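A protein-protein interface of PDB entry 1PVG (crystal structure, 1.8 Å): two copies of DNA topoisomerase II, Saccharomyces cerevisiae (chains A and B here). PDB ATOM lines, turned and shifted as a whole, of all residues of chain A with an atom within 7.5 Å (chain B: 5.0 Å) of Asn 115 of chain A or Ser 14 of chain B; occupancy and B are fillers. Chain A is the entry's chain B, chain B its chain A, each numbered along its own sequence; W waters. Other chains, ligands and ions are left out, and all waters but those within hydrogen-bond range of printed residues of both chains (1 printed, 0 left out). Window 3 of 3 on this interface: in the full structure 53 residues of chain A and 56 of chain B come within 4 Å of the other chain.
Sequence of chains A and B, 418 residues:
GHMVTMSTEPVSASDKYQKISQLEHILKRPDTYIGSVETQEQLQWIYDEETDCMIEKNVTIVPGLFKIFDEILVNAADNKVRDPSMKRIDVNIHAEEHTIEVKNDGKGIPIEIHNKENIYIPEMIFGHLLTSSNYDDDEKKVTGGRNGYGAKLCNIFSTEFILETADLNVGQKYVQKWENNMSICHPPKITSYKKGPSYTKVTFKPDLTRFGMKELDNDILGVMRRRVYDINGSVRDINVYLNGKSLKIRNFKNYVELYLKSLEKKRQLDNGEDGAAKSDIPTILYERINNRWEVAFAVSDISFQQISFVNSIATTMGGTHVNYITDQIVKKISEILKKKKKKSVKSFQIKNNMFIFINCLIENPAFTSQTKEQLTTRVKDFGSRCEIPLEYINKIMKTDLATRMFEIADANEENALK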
ATOM      1  N   PRO A 110      25.221  -0.520 -10.228  1.00  0.00           N
ATOM      2  CA  PRO A 110      26.442   0.216  -9.877  1.00  0.00           C
ATOM      3  C   PRO A 110      27.696  -0.625 -10.096  1.00  0.00           C
ATOM      4  O   PRO A 110      27.818  -1.702  -9.508  1.00  0.00           O
ATOM      5  CB  PRO A 110      26.248   0.507  -8.390  1.00  0.00           C
ATOM      6  CG  PRO A 110      24.775   0.617  -8.235  1.00  0.00           C
ATOM      7  CD  PRO A 110      24.195  -0.416  -9.172  1.00  0.00           C
ATOM      8  N   GLU A 112      30.822  -0.969  -8.995  1.00  0.00           N
ATOM      9  CA  GLU A 112      31.608  -0.591  -7.831  1.00  0.00           C
ATOM     10  C   GLU A 112      31.983  -1.850  -7.072  1.00  0.00           C
ATOM     11  O   GLU A 112      31.236  -2.830  -7.074  1.00  0.00           O
ATOM     12  CB  GLU A 112      30.783   0.302  -6.902  1.00  0.00           C
ATOM     13  CG  GLU A 112      30.741   1.771  -7.283  1.00  0.00           C
ATOM     14  CD  GLU A 112      29.679   2.533  -6.511  1.00  0.00           C
ATOM     15  OE1 GLU A 112      29.926   2.869  -5.331  1.00  0.00           O
ATOM     16  OE2 GLU A 112      28.593   2.789  -7.079  1.00  0.00           O
ATOM     17  N   ILE A 113      33.143  -1.820  -6.423  1.00  0.00           N
ATOM     18  CA  ILE A 113      33.493  -2.850  -5.451  1.00  0.00           C
ATOM     19  C   ILE A 113      32.783  -2.548  -4.130  1.00  0.00           C
ATOM     20  O   ILE A 113      32.864  -1.433  -3.614  1.00  0.00           O
ATOM     21  CB  ILE A 113      35.028  -2.927  -5.251  1.00  0.00           C
ATOM     22  CG1 ILE A 113      35.709  -3.411  -6.537  1.00  0.00           C
ATOM     23  CG2 ILE A 113      35.382  -3.842  -4.068  1.00  0.00           C
ATOM     24  CD1 ILE A 113      37.146  -2.960  -6.675  1.00  0.00           C
ATOM     25  N   HIS A 114      32.067  -3.543  -3.608  1.00  0.00           N
ATOM     26  CA  HIS A 114      31.363  -3.416  -2.336  1.00  0.00           C
ATOM     27  C   HIS A 114      32.338  -3.210  -1.170  1.00  0.00           C
ATOM     28  O   HIS A 114      33.392  -3.849  -1.120  1.00  0.00           O
ATOM     29  CB  HIS A 114      30.503  -4.660  -2.089  1.00  0.00           C
ATOM     30  CG  HIS A 114      29.437  -4.465  -1.057  1.00  0.00           C
ATOM     31  ND1 HIS A 114      29.655  -4.673   0.288  1.00  0.00           N
ATOM     32  CD2 HIS A 114      28.141  -4.089  -1.175  1.00  0.00           C
ATOM     33  CE1 HIS A 114      28.541  -4.430   0.955  1.00  0.00           C
ATOM     34  NE2 HIS A 114      27.606  -4.076   0.090  1.00  0.00           N
ATOM     35  N   ASN A 115      31.969  -2.321  -0.242  1.00  0.00           N
ATOM     36  CA  ASN A 115      32.769  -2.017   0.956  1.00  0.00           C
ATOM     37  C   ASN A 115      33.167  -3.247   1.767  1.00  0.00           C
ATOM     38  O   ASN A 115      34.322  -3.378   2.195  1.00  0.00           O
ATOM     39  CB  ASN A 115      31.995  -1.074   1.887  1.00  0.00           C
ATOM     40  CG  ASN A 115      32.014   0.364   1.419  1.00  0.00           C
ATOM     41  OD1 ASN A 115      32.614   0.694   0.393  1.00  0.00           O
ATOM     42  ND2 ASN A 115      31.340   1.233   2.167  1.00  0.00           N
ATOM     43  N   LYS A 116      32.191  -4.123   1.993  1.00  0.00           N
ATOM     44  CA  LYS A 116      32.329  -5.248   2.910  1.00  0.00           C
ATOM     45  C   LYS A 116      32.763  -6.529   2.210  1.00  0.00           C
ATOM     46  O   LYS A 116      33.655  -7.232   2.693  1.00  0.00           O
ATOM     47  CB  LYS A 116      31.009  -5.494   3.648  1.00  0.00           C
ATOM     48  CG  LYS A 116      30.725  -4.512   4.775  1.00  0.00           C
ATOM     49  CD  LYS A 116      29.541  -3.612   4.433  1.00  0.00           C
ATOM     50  CE  LYS A 116      28.898  -3.043   5.692  1.00  0.00           C
ATOM     51  NZ  LYS A 116      27.646  -2.284   5.390  1.00  0.00           N
ATOM     52  N   GLU A 117      32.135  -6.825   1.074  1.00  0.00           N
ATOM     53  CA  GLU A 117      32.330  -8.102   0.388  1.00  0.00           C
ATOM     54  C   GLU A 117      33.564  -8.107  -0.504  1.00  0.00           C
ATOM     55  O   GLU A 117      34.045  -9.173  -0.903  1.00  0.00           O
ATOM     56  CB  GLU A 117      31.082  -8.485  -0.423  1.00  0.00           C
ATOM     57  CG  GLU A 117      29.788  -8.549   0.387  1.00  0.00           C
ATOM     58  CD  GLU A 117      29.905  -9.409   1.633  1.00  0.00           C
ATOM     59  OE1 GLU A 117      30.562 -10.474   1.572  1.00  0.00           O
ATOM     60  OE2 GLU A 117      29.338  -9.017   2.680  1.00  0.00           O
ATOM     61  N   ASN A 118      34.061  -6.908  -0.813  1.00  0.00           N
ATOM     62  CA  ASN A 118      35.301  -6.708  -1.583  1.00  0.00           C
ATOM     63  C   ASN A 118      35.301  -7.373  -2.963  1.00  0.00           C
ATOM     64  O   ASN A 118      36.337  -7.824  -3.454  1.00  0.00           O
ATOM     65  CB  ASN A 118      36.539  -7.119  -0.766  1.00  0.00           C
ATOM     66  CG  ASN A 118      36.494  -6.602   0.661  1.00  0.00           C
ATOM     67  OD1 ASN A 118      36.795  -5.435   0.926  1.00  0.00           O
ATOM     68  ND2 ASN A 118      36.115  -7.472   1.591  1.00  0.00           N
ATOM     69  N   ILE A 119      34.119  -7.444  -3.569  1.00  0.00           N
ATOM     70  CA  ILE A 119      33.964  -7.866  -4.957  1.00  0.00           C
ATOM     71  C   ILE A 119      33.009  -6.888  -5.633  1.00  0.00           C
ATOM     72  O   ILE A 119      32.291  -6.145  -4.951  1.00  0.00           O
ATOM     73  CB  ILE A 119      33.394  -9.313  -5.042  1.00  0.00           C
ATOM     74  CG1 ILE A 119      32.117  -9.445  -4.199  1.00  0.00           C
ATOM     75  CG2 ILE A 119      34.445 -10.347  -4.642  1.00  0.00           C
ATOM     76  CD1 ILE A 119      31.342 -10.720  -4.446  1.00  0.00           C
ATOM     77  N   ILE A 121      29.813  -5.299  -7.183  1.00  0.00           N
ATOM     78  CA  ILE A 121      28.424  -5.436  -6.752  1.00  0.00           C
ATOM     79  C   ILE A 121      27.584  -6.336  -7.671  1.00  0.00           C
ATOM     80  O   ILE A 121      26.835  -7.172  -7.174  1.00  0.00           O
ATOM     81  CB  ILE A 121      27.768  -4.041  -6.508  1.00  0.00           C
ATOM     82  CG1 ILE A 121      28.189  -3.506  -5.131  1.00  0.00           C
ATOM     83  CG2 ILE A 121      26.235  -4.110  -6.628  1.00  0.00           C
ATOM     84  CD1 ILE A 121      28.060  -2.010  -4.970  1.00  0.00           C
ATOM     85  N   MET A 124      28.354  -9.750  -6.851  1.00  0.00           N
ATOM     86  CA  MET A 124      27.812 -10.039  -5.536  1.00  0.00           C
ATOM     87  C   MET A 124      26.328 -10.408  -5.601  1.00  0.00           C
ATOM     88  O   MET A 124      25.917 -11.433  -5.067  1.00  0.00           O
ATOM     89  CB  MET A 124      28.023  -8.840  -4.615  1.00  0.00           C
ATOM     90  CG  MET A 124      27.513  -9.033  -3.195  1.00  0.00           C
ATOM     91  SD  MET A 124      27.499  -7.317  -2.263  1.00  0.00           S
ATOM     92  CE  MET A 124      25.811  -7.486  -1.315  1.00  0.00           C
ATOM     93  N   SER B  12      26.902   4.428   0.109  1.00  0.00           N
ATOM     94  CA  SER B  12      25.426   4.275  -0.039  1.00  0.00           C
ATOM     95  C   SER B  12      25.060   3.059  -0.891  1.00  0.00           C
ATOM     96  O   SER B  12      24.131   2.335  -0.559  1.00  0.00           O
ATOM     97  CB  SER B  12      24.791   5.539  -0.627  1.00  0.00           C
ATOM     98  OG  SER B  12      23.393   5.356  -0.820  1.00  0.00           O
ATOM     99  N   ALA B  13      25.786   2.854  -1.991  1.00  0.00           N
ATOM    100  CA  ALA B  13      25.596   1.674  -2.839  1.00  0.00           C
ATOM    101  C   ALA B  13      26.004   0.410  -2.094  1.00  0.00           C
ATOM    102  O   ALA B  13      25.375  -0.644  -2.239  1.00  0.00           O
ATOM    103  CB  ALA B  13      26.388   1.813  -4.132  1.00  0.00           C
ATOM    104  N   SER B  14      27.053   0.526  -1.283  1.00  0.00           N
ATOM    105  CA  SER B  14      27.478  -0.555  -0.404  1.00  0.00           C
ATOM    106  C   SER B  14      26.469  -0.786   0.717  1.00  0.00           C
ATOM    107  O   SER B  14      26.312  -1.915   1.202  1.00  0.00           O
ATOM    108  CB  SER B  14      28.849  -0.245   0.186  1.00  0.00           C
ATOM    109  OG  SER B  14      29.879  -0.708  -0.666  1.00  0.00           O
ATOM    110  N   ASP B  15      25.798   0.287   1.130  1.00  0.00           N
ATOM    111  CA  ASP B  15      24.758   0.203   2.153  1.00  0.00           C
ATOM    112  C   ASP B  15      23.446  -0.289   1.553  1.00  0.00           C
ATOM    113  O   ASP B  15      22.637  -0.900   2.246  1.00  0.00           O
ATOM    114  CB  ASP B  15      24.543   1.563   2.826  1.00  0.00           C
ATOM    115  CG  ASP B  15      25.574   1.856   3.915  1.00  0.00           C
ATOM    116  OD1 ASP B  15      26.132   0.903   4.499  1.00  0.00           O
ATOM    117  OD2 ASP B  15      25.883   3.019   4.252  1.00  0.00           O
ATOM    118  N   LYS B  16      23.248  -0.018   0.265  1.00  0.00           N
ATOM    119  CA  LYS B  16      22.008  -0.370  -0.433  1.00  0.00           C
ATOM    120  C   LYS B  16      21.905  -1.872  -0.694  1.00  0.00           C
ATOM    121  O   LYS B  16      20.845  -2.466  -0.509  1.00  0.00           O
ATOM    122  CB  LYS B  16      21.888   0.412  -1.748  1.00  0.00           C
ATOM    123  CG  LYS B  16      20.798  -0.090  -2.692  1.00  0.00           C
ATOM    124  CD  LYS B  16      19.784   1.002  -3.012  1.00  0.00           C
ATOM    125  CE  LYS B  16      18.653   0.463  -3.880  1.00  0.00           C
ATOM    126  NZ  LYS B  16      18.874   0.764  -5.323  1.00  0.00           N
ATOM    127  N   TYR B  17      23.009  -2.472  -1.132  1.00  0.00           N
ATOM    128  CA  TYR B  17      23.062  -3.905  -1.411  1.00  0.00           C
ATOM    129  C   TYR B  17      23.695  -4.651  -0.250  1.00  0.00           C
ATOM    130  O   TYR B  17      24.815  -4.338   0.162  1.00  0.00           O
ATOM    131  CB  TYR B  17      23.826  -4.173  -2.714  1.00  0.00           C
ATOM    132  CG  TYR B  17      23.250  -3.428  -3.895  1.00  0.00           C
ATOM    133  CD1 TYR B  17      22.201  -3.965  -4.644  1.00  0.00           C
ATOM    134  CD2 TYR B  17      23.729  -2.170  -4.244  1.00  0.00           C
ATOM    135  CE1 TYR B  17      21.663  -3.271  -5.719  1.00  0.00           C
ATOM    136  CE2 TYR B  17      23.198  -1.471  -5.314  1.00  0.00           C
ATOM    137  CZ  TYR B  17      22.166  -2.025  -6.046  1.00  0.00           C
ATOM    138  OH  TYR B  17      21.650  -1.321  -7.111  1.00  0.00           O
HETATM  139  O   HOH W   1      25.684  -3.558   3.225  1.00  0.00           O
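The backbone carbonyl oxygen (O) of Ser 14 of chain B is in hydrogen-bond range of a ring nitrogen (NE2) of His 114 of chain A, 2.8 Å away.
The side-chain hydroxyl (OG) of Ser 14 of chain B sits at hydrogen-bond distance from the backbone NH (N) of Asn 115 of chain A (2.7 Å).
The side-chain carboxylate (OD1) of Asp 15 of chain B is in salt-bridge range of the side-chain amino group (NZ) of Lys 116 of chain A.
O of Tyr 17 of chain B is in hydrogen-bond range of NE2 of His 114 of chain A, at 2.8 Å.
O of Glu 112 of chain A is in hydrogen-bond range of N of Ile 121 of chain A (2.9 Å).
The backbone NH (N) of Lys 116 of chain A lies within hydrogen-bond range of a ring nitrogen (ND1) of His 114 of chain A (3.1 Å).
A ring nitrogen (ND1) of His 114 of chain A lies within hydrogen-bond range of the backbone NH of Glu 117 of chain A.
N of His 114 of chain A lies within hydrogen-bond range of O of Ile 119 of chain A, 2.9 Å away.
The backbone carbonyl oxygen (O) of Asn 115 of chain A lies close to the side-chain amide oxygen (OD1) of Asn 118 of chain A (3.5 Å).
O of Lys 116 of chain A sits at hydrogen-bond distance from ND2 of Asn 118 of chain A (2.7 Å).
Among the printed residues, pairs that only touch across the chains: Pro 110 of chain A with Tyr 17 of chain B, Met 124 of chain A with Tyr 17 of chain B, Glu 112 of chain A with Ala 13 of chain B and Ile 121 of chain A with Tyr 17 of chain B.
Asn 115 of chain A touches one residue of chain B.
Ser 14 of chain B touches just these residues of chain A: His 114 and Asn 115.
Of the printed residues of chain B, Lys 116 of chain A touches Asp 15 (3.6 Å).
Printed residues of chain B within 4 Å of His 114 of chain A: Ser 14 and Tyr 17.
Asn 118 of chain A touches none of the printed residues of chain B.
The nearest printed residue of chain B that does not touch Asn 115 of chain A is Asp 15 of chain B (5.7 Å).
The nearest residue of chain A that does not touch Ser 14 of chain B is Ile 113 of chain A (4.3 Å).
The nearest printed residue of chain B that does not touch Met 124 of chain A is Ser 14 of chain B (6.1 Å).
Of the 6 printed residues of chain B, 4 touch a printed residue of chain A.
Hydrophobic or aromatic side chains of chain B within 4 Å of the printed part of chain A: Ala 13 and Tyr 17.
Along chain B the printed residues that touch a printed residue of chain A span positions 13 to 17.
Hydrophobic or aromatic side chains of chain A that line the printed part of chain B: Pro 110, His 114, Ile 121 and Met 124.
Among the printed residues, 8 pairs touch across the chains.
No position is printed for both chains.
Water W1 lies within hydrogen-bond range of the backbone carbonyl oxygen (O) of Ser 14 of chain B (2.7 Å), the side-chain amino group (NZ) of Lys 116 of chain A (3.2 Å) and the backbone carbonyl oxygen (O) of Tyr 17 of chain B (3.3 Å).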
